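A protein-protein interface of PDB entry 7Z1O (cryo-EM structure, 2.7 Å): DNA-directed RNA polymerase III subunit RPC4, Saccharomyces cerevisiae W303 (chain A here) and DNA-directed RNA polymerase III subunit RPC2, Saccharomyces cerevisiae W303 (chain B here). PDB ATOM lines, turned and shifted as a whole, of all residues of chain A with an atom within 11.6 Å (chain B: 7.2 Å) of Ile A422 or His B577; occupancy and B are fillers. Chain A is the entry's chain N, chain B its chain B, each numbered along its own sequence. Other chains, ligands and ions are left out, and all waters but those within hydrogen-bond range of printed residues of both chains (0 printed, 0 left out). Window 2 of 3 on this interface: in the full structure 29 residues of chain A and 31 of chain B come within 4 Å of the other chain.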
ATOM      1  N   PRO A 310      36.894 -12.176  30.471  1.00  0.00           N
ATOM      2  CA  PRO A 310      36.001 -13.284  30.116  1.00  0.00           C
ATOM      3  C   PRO A 310      36.408 -14.579  30.806  1.00  0.00           C
ATOM      4  O   PRO A 310      37.594 -14.856  30.999  1.00  0.00           O
ATOM      5  CB  PRO A 310      36.151 -13.386  28.592  1.00  0.00           C
ATOM      6  CG  PRO A 310      37.356 -12.577  28.247  1.00  0.00           C
ATOM      7  CD  PRO A 310      37.418 -11.502  29.272  1.00  0.00           C
ATOM      8  N   VAL A 373      41.977  -3.802  24.618  1.00  0.00           N
ATOM      9  CA  VAL A 373      42.736  -4.895  25.212  1.00  0.00           C
ATOM     10  C   VAL A 373      42.814  -6.014  24.185  1.00  0.00           C
ATOM     11  O   VAL A 373      41.799  -6.629  23.844  1.00  0.00           O
ATOM     12  CB  VAL A 373      42.100  -5.379  26.520  1.00  0.00           C
ATOM     13  CG1 VAL A 373      42.925  -6.498  27.125  1.00  0.00           C
ATOM     14  CG2 VAL A 373      41.961  -4.223  27.497  1.00  0.00           C
ATOM     15  N   VAL A 378      42.400 -11.483  19.453  1.00  0.00           N
ATOM     16  CA  VAL A 378      41.095 -10.829  19.508  1.00  0.00           C
ATOM     17  C   VAL A 378      41.225  -9.509  20.258  1.00  0.00           C
ATOM     18  O   VAL A 378      41.977  -9.403  21.236  1.00  0.00           O
ATOM     19  CB  VAL A 378      40.018 -11.735  20.135  1.00  0.00           C
ATOM     20  CG1 VAL A 378      39.859 -13.006  19.323  1.00  0.00           C
ATOM     21  CG2 VAL A 378      40.334 -12.075  21.567  1.00  0.00           C
ATOM     22  N   VAL A 379      40.517  -8.498  19.774  1.00  0.00           N
ATOM     23  CA  VAL A 379      40.491  -7.172  20.378  1.00  0.00           C
ATOM     24  C   VAL A 379      39.215  -7.033  21.194  1.00  0.00           C
ATOM     25  O   VAL A 379      38.129  -7.426  20.760  1.00  0.00           O
ATOM     26  CB  VAL A 379      40.599  -6.076  19.297  1.00  0.00           C
ATOM     27  CG1 VAL A 379      40.725  -4.702  19.935  1.00  0.00           C
ATOM     28  CG2 VAL A 379      41.777  -6.356  18.380  1.00  0.00           C
ATOM     29  N   MET A 380      39.344  -6.475  22.397  1.00  0.00           N
ATOM     30  CA  MET A 380      38.239  -6.350  23.331  1.00  0.00           C
ATOM     31  C   MET A 380      38.156  -4.913  23.823  1.00  0.00           C
ATOM     32  O   MET A 380      39.167  -4.212  23.918  1.00  0.00           O
ATOM     33  CB  MET A 380      38.409  -7.294  24.530  1.00  0.00           C
ATOM     34  CG  MET A 380      38.913  -8.692  24.198  1.00  0.00           C
ATOM     35  SD  MET A 380      38.636  -9.840  25.561  1.00  0.00           S
ATOM     36  CE  MET A 380      38.659 -11.414  24.723  1.00  0.00           C
ATOM     37  N   ASP A 381      36.936  -4.485  24.139  1.00  0.00           N
ATOM     38  CA  ASP A 381      36.704  -3.164  24.697  1.00  0.00           C
ATOM     39  C   ASP A 381      36.924  -3.192  26.207  1.00  0.00           C
ATOM     40  O   ASP A 381      36.903  -4.247  26.848  1.00  0.00           O
ATOM     41  CB  ASP A 381      35.296  -2.684  24.352  1.00  0.00           C
ATOM     42  CG  ASP A 381      35.018  -2.714  22.862  1.00  0.00           C
ATOM     43  OD1 ASP A 381      35.988  -2.736  22.075  1.00  0.00           O
ATOM     44  OD2 ASP A 381      33.830  -2.716  22.478  1.00  0.00           O
ATOM     45  N   ILE A 382      37.129  -2.015  26.788  1.00  0.00           N
ATOM     46  CA  ILE A 382      37.454  -1.894  28.206  1.00  0.00           C
ATOM     47  C   ILE A 382      36.589  -0.793  28.810  1.00  0.00           C
ATOM     48  O   ILE A 382      36.404   0.268  28.205  1.00  0.00           O
ATOM     49  CB  ILE A 382      38.961  -1.623  28.407  1.00  0.00           C
ATOM     50  CG1 ILE A 382      39.294  -1.355  29.874  1.00  0.00           C
ATOM     51  CG2 ILE A 382      39.431  -0.485  27.523  1.00  0.00           C
ATOM     52  CD1 ILE A 382      40.774  -1.395  30.160  1.00  0.00           C
ATOM     53  N   VAL A 418      36.822  -6.040  30.941  1.00  0.00           N
ATOM     54  CA  VAL A 418      37.246  -6.271  29.567  1.00  0.00           C
ATOM     55  C   VAL A 418      36.205  -7.152  28.892  1.00  0.00           C
ATOM     56  O   VAL A 418      35.958  -8.283  29.331  1.00  0.00           O
ATOM     57  CB  VAL A 418      38.641  -6.914  29.526  1.00  0.00           C
ATOM     58  CG1 VAL A 418      38.953  -7.418  28.143  1.00  0.00           C
ATOM     59  CG2 VAL A 418      39.693  -5.920  29.985  1.00  0.00           C
ATOM     60  N   THR A 419      35.588  -6.637  27.828  1.00  0.00           N
ATOM     61  CA  THR A 419      34.461  -7.295  27.182  1.00  0.00           C
ATOM     62  C   THR A 419      34.761  -7.550  25.712  1.00  0.00           C
ATOM     63  O   THR A 419      35.281  -6.665  25.024  1.00  0.00           O
ATOM     64  CB  THR A 419      33.187  -6.443  27.284  1.00  0.00           C
ATOM     65  OG1 THR A 419      33.333  -5.268  26.478  1.00  0.00           O
ATOM     66  CG2 THR A 419      32.938  -6.021  28.715  1.00  0.00           C
ATOM     67  N   PRO A 420      34.440  -8.739  25.201  1.00  0.00           N
ATOM     68  CA  PRO A 420      34.596  -8.989  23.763  1.00  0.00           C
ATOM     69  C   PRO A 420      33.718  -8.059  22.940  1.00  0.00           C
ATOM     70  O   PRO A 420      32.577  -7.768  23.305  1.00  0.00           O
ATOM     71  CB  PRO A 420      34.160 -10.449  23.611  1.00  0.00           C
ATOM     72  CG  PRO A 420      34.384 -11.047  24.957  1.00  0.00           C
ATOM     73  CD  PRO A 420      34.039  -9.955  25.927  1.00  0.00           C
ATOM     74  N   GLN A 421      34.257  -7.594  21.817  1.00  0.00           N
ATOM     75  CA  GLN A 421      33.516  -6.728  20.910  1.00  0.00           C
ATOM     76  C   GLN A 421      32.805  -7.593  19.877  1.00  0.00           C
ATOM     77  O   GLN A 421      33.314  -8.649  19.483  1.00  0.00           O
ATOM     78  CB  GLN A 421      34.437  -5.711  20.236  1.00  0.00           C
ATOM     79  CG  GLN A 421      35.452  -6.296  19.271  1.00  0.00           C
ATOM     80  CD  GLN A 421      36.319  -5.234  18.627  1.00  0.00           C
ATOM     81  OE1 GLN A 421      36.144  -4.041  18.872  1.00  0.00           O
ATOM     82  NE2 GLN A 421      37.262  -5.663  17.797  1.00  0.00           N
ATOM     83  N   ILE A 422      31.618  -7.163  19.464  1.00  0.00           N
ATOM     84  CA  ILE A 422      30.823  -7.928  18.516  1.00  0.00           C
ATOM     85  C   ILE A 422      30.493  -7.075  17.297  1.00  0.00           C
ATOM     86  O   ILE A 422      29.919  -5.993  17.423  1.00  0.00           O
ATOM     87  CB  ILE A 422      29.540  -8.463  19.170  1.00  0.00           C
ATOM     88  CG1 ILE A 422      29.870  -9.229  20.449  1.00  0.00           C
ATOM     89  CG2 ILE A 422      28.803  -9.374  18.215  1.00  0.00           C
ATOM     90  CD1 ILE A 422      28.662  -9.613  21.249  1.00  0.00           C
ATOM     91  N   LEU B 532      26.783 -15.877  29.043  1.00  0.00           N
ATOM     92  CA  LEU B 532      26.934 -14.853  28.015  1.00  0.00           C
ATOM     93  C   LEU B 532      26.762 -13.456  28.600  1.00  0.00           C
ATOM     94  O   LEU B 532      27.452 -12.512  28.196  1.00  0.00           O
ATOM     95  CB  LEU B 532      25.940 -15.092  26.882  1.00  0.00           C
ATOM     96  CG  LEU B 532      26.180 -14.233  25.644  1.00  0.00           C
ATOM     97  CD1 LEU B 532      27.300 -14.824  24.808  1.00  0.00           C
ATOM     98  CD2 LEU B 532      24.910 -14.111  24.831  1.00  0.00           C
ATOM     99  N   LEU B 536      29.722 -10.683  28.545  1.00  0.00           N
ATOM    100  CA  LEU B 536      29.487  -9.419  27.853  1.00  0.00           C
ATOM    101  C   LEU B 536      29.741  -8.192  28.722  1.00  0.00           C
ATOM    102  O   LEU B 536      29.785  -7.081  28.186  1.00  0.00           O
ATOM    103  CB  LEU B 536      28.064  -9.362  27.299  1.00  0.00           C
ATOM    104  CG  LEU B 536      27.839 -10.145  26.005  1.00  0.00           C
ATOM    105  CD1 LEU B 536      26.397 -10.035  25.547  1.00  0.00           C
ATOM    106  CD2 LEU B 536      28.786  -9.659  24.930  1.00  0.00           C
ATOM    107  N   LYS B 570      24.677  -0.488  24.641  1.00  0.00           N
ATOM    108  CA  LYS B 570      25.667  -1.311  23.955  1.00  0.00           C
ATOM    109  C   LYS B 570      25.452  -2.790  24.247  1.00  0.00           C
ATOM    110  O   LYS B 570      25.604  -3.635  23.356  1.00  0.00           O
ATOM    111  CB  LYS B 570      27.078  -0.885  24.357  1.00  0.00           C
ATOM    112  CG  LYS B 570      28.167  -1.449  23.463  1.00  0.00           C
ATOM    113  CD  LYS B 570      29.523  -1.407  24.142  1.00  0.00           C
ATOM    114  CE  LYS B 570      30.042   0.016  24.246  1.00  0.00           C
ATOM    115  NZ  LYS B 570      31.035   0.163  25.345  1.00  0.00           N
ATOM    116  N   PHE B 571      25.094  -3.119  25.490  1.00  0.00           N
ATOM    117  CA  PHE B 571      24.796  -4.500  25.855  1.00  0.00           C
ATOM    118  C   PHE B 571      23.598  -5.027  25.074  1.00  0.00           C
ATOM    119  O   PHE B 571      23.625  -6.149  24.551  1.00  0.00           O
ATOM    120  CB  PHE B 571      24.545  -4.581  27.361  1.00  0.00           C
ATOM    121  CG  PHE B 571      24.189  -5.949  27.852  1.00  0.00           C
ATOM    122  CD1 PHE B 571      25.150  -6.937  27.943  1.00  0.00           C
ATOM    123  CD2 PHE B 571      22.898  -6.239  28.247  1.00  0.00           C
ATOM    124  CE1 PHE B 571      24.825  -8.194  28.403  1.00  0.00           C
ATOM    125  CE2 PHE B 571      22.568  -7.493  28.710  1.00  0.00           C
ATOM    126  CZ  PHE B 571      23.533  -8.470  28.788  1.00  0.00           C
ATOM    127  N   VAL B 572      22.546  -4.212  24.964  1.00  0.00           N
ATOM    128  CA  VAL B 572      21.352  -4.606  24.222  1.00  0.00           C
ATOM    129  C   VAL B 572      21.675  -4.793  22.743  1.00  0.00           C
ATOM    130  O   VAL B 572      21.233  -5.763  22.114  1.00  0.00           O
ATOM    131  CB  VAL B 572      20.233  -3.570  24.440  1.00  0.00           C
ATOM    132  CG1 VAL B 572      19.137  -3.725  23.408  1.00  0.00           C
ATOM    133  CG2 VAL B 572      19.661  -3.702  25.837  1.00  0.00           C
ATOM    134  N   THR B 573      22.463  -3.877  22.171  1.00  0.00           N
ATOM    135  CA  THR B 573      22.826  -3.974  20.760  1.00  0.00           C
ATOM    136  C   THR B 573      23.670  -5.213  20.484  1.00  0.00           C
ATOM    137  O   THR B 573      23.443  -5.919  19.494  1.00  0.00           O
ATOM    138  CB  THR B 573      23.566  -2.708  20.327  1.00  0.00           C
ATOM    139  OG1 THR B 573      22.671  -1.591  20.384  1.00  0.00           O
ATOM    140  CG2 THR B 573      24.098  -2.843  18.910  1.00  0.00           C
ATOM    141  N   GLN B 574      24.638  -5.505  21.357  1.00  0.00           N
ATOM    142  CA  GLN B 574      25.470  -6.691  21.176  1.00  0.00           C
ATOM    143  C   GLN B 574      24.655  -7.972  21.323  1.00  0.00           C
ATOM    144  O   GLN B 574      24.865  -8.939  20.578  1.00  0.00           O
ATOM    145  CB  GLN B 574      26.626  -6.670  22.172  1.00  0.00           C
ATOM    146  CG  GLN B 574      27.733  -5.697  21.808  1.00  0.00           C
ATOM    147  CD  GLN B 574      28.886  -5.736  22.787  1.00  0.00           C
ATOM    148  OE1 GLN B 574      28.683  -5.816  23.997  1.00  0.00           O
ATOM    149  NE2 GLN B 574      30.106  -5.682  22.268  1.00  0.00           N
ATOM    150  N   PHE B 575      23.719  -7.997  22.275  1.00  0.00           N
ATOM    151  CA  PHE B 575      22.866  -9.169  22.441  1.00  0.00           C
ATOM    152  C   PHE B 575      21.966  -9.373  21.227  1.00  0.00           C
ATOM    153  O   PHE B 575      21.771 -10.508  20.774  1.00  0.00           O
ATOM    154  CB  PHE B 575      22.035  -9.026  23.713  1.00  0.00           C
ATOM    155  CG  PHE B 575      21.587 -10.330  24.294  1.00  0.00           C
ATOM    156  CD1 PHE B 575      22.402 -11.027  25.166  1.00  0.00           C
ATOM    157  CD2 PHE B 575      20.353 -10.864  23.966  1.00  0.00           C
ATOM    158  CE1 PHE B 575      21.995 -12.227  25.706  1.00  0.00           C
ATOM    159  CE2 PHE B 575      19.942 -12.067  24.501  1.00  0.00           C
ATOM    160  CZ  PHE B 575      20.765 -12.749  25.372  1.00  0.00           C
ATOM    161  N   ARG B 576      21.419  -8.283  20.676  1.00  0.00           N
ATOM    162  CA  ARG B 576      20.617  -8.384  19.461  1.00  0.00           C
ATOM    163  C   ARG B 576      21.456  -8.853  18.282  1.00  0.00           C
ATOM    164  O   ARG B 576      20.978  -9.616  17.436  1.00  0.00           O
ATOM    165  CB  ARG B 576      19.962  -7.041  19.139  1.00  0.00           C
ATOM    166  CG  ARG B 576      18.797  -6.669  20.032  1.00  0.00           C
ATOM    167  CD  ARG B 576      18.058  -5.461  19.482  1.00  0.00           C
ATOM    168  NE  ARG B 576      17.558  -4.587  20.535  1.00  0.00           N
ATOM    169  CZ  ARG B 576      16.410  -4.762  21.174  1.00  0.00           C
ATOM    170  NH1 ARG B 576      15.623  -5.789  20.905  1.00  0.00           N
ATOM    171  NH2 ARG B 576      16.041  -3.885  22.101  1.00  0.00           N
ATOM    172  N   HIS B 577      22.707  -8.394  18.200  1.00  0.00           N
ATOM    173  CA  HIS B 577      23.597  -8.843  17.134  1.00  0.00           C
ATOM    174  C   HIS B 577      23.876 -10.335  17.243  1.00  0.00           C
ATOM    175  O   HIS B 577      23.896 -11.047  16.232  1.00  0.00           O
ATOM    176  CB  HIS B 577      24.904  -8.050  17.176  1.00  0.00           C
ATOM    177  CG  HIS B 577      25.793  -8.281  15.995  1.00  0.00           C
ATOM    178  ND1 HIS B 577      26.531  -9.433  15.831  1.00  0.00           N
ATOM    179  CD2 HIS B 577      26.073  -7.501  14.925  1.00  0.00           C
ATOM    180  CE1 HIS B 577      27.223  -9.356  14.709  1.00  0.00           C
ATOM    181  NE2 HIS B 577      26.962  -8.193  14.140  1.00  0.00           N
ATOM    182  N   LEU B 578      24.092 -10.827  18.466  1.00  0.00           N
ATOM    183  CA  LEU B 578      24.301 -12.259  18.658  1.00  0.00           C
ATOM    184  C   LEU B 578      23.048 -13.053  18.313  1.00  0.00           C
ATOM    185  O   LEU B 578      23.137 -14.160  17.769  1.00  0.00           O
ATOM    186  CB  LEU B 578      24.731 -12.546  20.095  1.00  0.00           C
ATOM    187  CG  LEU B 578      26.185 -12.210  20.418  1.00  0.00           C
ATOM    188  CD1 LEU B 578      26.551 -12.708  21.800  1.00  0.00           C
ATOM    189  CD2 LEU B 578      27.114 -12.791  19.369  1.00  0.00           C
ATOM    190  N   ARG B 579      21.873 -12.511  18.638  1.00  0.00           N
ATOM    191  CA  ARG B 579      20.626 -13.184  18.286  1.00  0.00           C
ATOM    192  C   ARG B 579      20.433 -13.249  16.776  1.00  0.00           C
ATOM    193  O   ARG B 579      20.013 -14.281  16.241  1.00  0.00           O
ATOM    194  CB  ARG B 579      19.446 -12.474  18.944  1.00  0.00           C
ATOM    195  CG  ARG B 579      18.157 -13.253  18.884  1.00  0.00           C
ATOM    196  CD  ARG B 579      17.080 -12.571  19.694  1.00  0.00           C
ATOM    197  NE  ARG B 579      16.587 -11.366  19.044  1.00  0.00           N
ATOM    198  CZ  ARG B 579      15.848 -10.444  19.643  1.00  0.00           C
ATOM    199  NH1 ARG B 579      15.498 -10.558  20.913  1.00  0.00           N
ATOM    200  NH2 ARG B 579      15.450  -9.380  18.952  1.00  0.00           N
ATOM    201  N   ARG B 580      20.729 -12.154  16.072  1.00  0.00           N
ATOM    202  CA  ARG B 580      20.525 -12.126  14.629  1.00  0.00           C
ATOM    203  C   ARG B 580      21.562 -12.963  13.893  1.00  0.00           C
ATOM    204  O   ARG B 580      21.258 -13.540  12.843  1.00  0.00           O
ATOM    205  CB  ARG B 580      20.543 -10.686  14.122  1.00  0.00           C
ATOM    206  CG  ARG B 580      19.367  -9.861  14.605  1.00  0.00           C
ATOM    207  CD  ARG B 580      19.625  -8.379  14.455  1.00  0.00           C
ATOM    208  NE  ARG B 580      18.521  -7.588  14.984  1.00  0.00           N
ATOM    209  CZ  ARG B 580      18.404  -6.277  14.840  1.00  0.00           C
ATOM    210  NH1 ARG B 580      19.311  -5.570  14.187  1.00  0.00           N
ATOM    211  NH2 ARG B 580      17.350  -5.659  15.363  1.00  0.00           N
ATOM    212  N   THR B 581      22.785 -13.038  14.417  1.00  0.00           N
ATOM    213  CA  THR B 581      23.802 -13.893  13.820  1.00  0.00           C
ATOM    214  C   THR B 581      23.493 -15.373  14.013  1.00  0.00           C
ATOM    215  O   THR B 581      23.719 -16.168  13.094  1.00  0.00           O
ATOM    216  CB  THR B 581      25.175 -13.552  14.408  1.00  0.00           C
ATOM    217  OG1 THR B 581      25.483 -12.180  14.131  1.00  0.00           O
ATOM    218  CG2 THR B 581      26.264 -14.422  13.803  1.00  0.00           C
ATOM    219  N   GLY B 582      22.945 -15.752  15.162  1.00  0.00           N
ATOM    220  CA  GLY B 582      22.592 -17.128  15.431  1.00  0.00           C
ATOM    221  C   GLY B 582      23.321 -17.773  16.586  1.00  0.00           C
ATOM    222  O   GLY B 582      23.195 -18.988  16.771  1.00  0.00           O
ATOM    223  N   LYS B 583      24.077 -17.004  17.368  1.00  0.00           N
ATOM    224  CA  LYS B 583      24.844 -17.568  18.470  1.00  0.00           C
ATOM    225  C   LYS B 583      23.978 -17.925  19.669  1.00  0.00           C
ATOM    226  O   LYS B 583      24.386 -18.760  20.483  1.00  0.00           O
ATOM    227  CB  LYS B 583      25.946 -16.594  18.894  1.00  0.00           C
ATOM    228  CG  LYS B 583      27.292 -16.855  18.229  1.00  0.00           C
ATOM    229  CD  LYS B 583      27.251 -16.569  16.735  1.00  0.00           C
ATOM    230  CE  LYS B 583      28.544 -16.981  16.055  1.00  0.00           C
ATOM    231  NZ  LYS B 583      28.447 -16.896  14.573  1.00  0.00           N
ATOM    232  N   VAL B 584      22.800 -17.314  19.800  1.00  0.00           N
ATOM    233  CA  VAL B 584      21.839 -17.668  20.834  1.00  0.00           C
ATOM    234  C   VAL B 584      20.506 -17.957  20.161  1.00  0.00           C
ATOM    235  O   VAL B 584      20.342 -17.776  18.952  1.00  0.00           O
ATOM    236  CB  VAL B 584      21.675 -16.566  21.904  1.00  0.00           C
ATOM    237  CG1 VAL B 584      22.966 -16.380  22.673  1.00  0.00           C
ATOM    238  CG2 VAL B 584      21.242 -15.265  21.266  1.00  0.00           C
ATOM    239  N   GLU B 647      13.212 -11.106  12.374  1.00  0.00           N
ATOM    240  CA  GLU B 647      13.406 -11.561  13.743  1.00  0.00           C
ATOM    241  C   GLU B 647      12.076 -11.568  14.479  1.00  0.00           C
ATOM    242  O   GLU B 647      11.137 -10.858  14.117  1.00  0.00           O
ATOM    243  CB  GLU B 647      14.426 -10.696  14.490  1.00  0.00           C
ATOM    244  CG  GLU B 647      13.978  -9.278  14.770  1.00  0.00           C
ATOM    245  CD  GLU B 647      14.945  -8.541  15.676  1.00  0.00           C
ATOM    246  OE1 GLU B 647      15.891  -9.179  16.182  1.00  0.00           O
ATOM    247  OE2 GLU B 647      14.763  -7.324  15.883  1.00  0.00           O
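Of chain B, only Leu B536, Gln B574, His B577 and Leu B578 come within 4 Å of Ile A422.
His B577 touches just one residue of chain A: Ile A422.
No residue of chain A comes within 4 Å of Thr B573.
Of chain A, only Ile A422 (3.7 Å) comes within 4 Å of Leu B578.
Thr B581 touches none of the printed residues of chain A.
Of the printed residues of chain A, Leu B536 touches Thr A419 and Ile A422.
Of the printed residues of chain B, Thr A419 touches Leu B536.
Lys B583 touches none of the printed residues of chain A.
Lys B570 touches none of the printed residues of chain A.
The nearest residue of chain B that does not touch Ile A422 is Phe B575 (5.3 Å).
The nearest residue of chain A that does not touch His B577 is Gln A421 (7.7 Å).
The nearest printed residue of chain B that does not touch Pro A420 is Leu B536 (4.5 Å).
Hydrophobic or aromatic side chains of chain A that line the printed part of chain B: Ile A422.
Of the 18 printed residues of chain B, 4 touch a printed residue of chain A.
Hydrophobic or aromatic side chains of chain B that line the printed part of chain A: Leu B536, His B577 and Leu B578.
Among the printed residues, 7 pairs touch across the chains.
Among the printed residues, no Asp or Glu carboxylate lies within 4 Å of a Lys or Arg side-chain nitrogen of the other chain.
The backbone carbonyl oxygen of Leu B578 is in hydrogen-bond range of the backbone NH of Lys B583.
The side-chain carboxylate (OD1) of Asp A381 sits close to the side-chain amide oxygen (OE1) of Gln A421 (3.5 Å).
N of Asp A381 lies within hydrogen-bond range of O of Thr A419 (2.9 Å).
The backbone carbonyl oxygen (O) of His B577 lies within hydrogen-bond range of the side-chain hydroxyl (OG1) of Thr B581.
Among the printed residues, pairs that only touch across the chains: Ile A422 with His B577 (3.3 Å), Thr A419 with Leu B536 (3.4 Å), Ile A422 with Gln B574 (3.5 Å), Ile A422 with Leu B536 (3.7 Å), Ile A422 with Leu B578 (3.7 Å) and Gln A421 with Gln B574 (3.8 Å).
O of Pro A420 lies within hydrogen-bond range of NE2 of Gln B574, at 3.4 Å.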
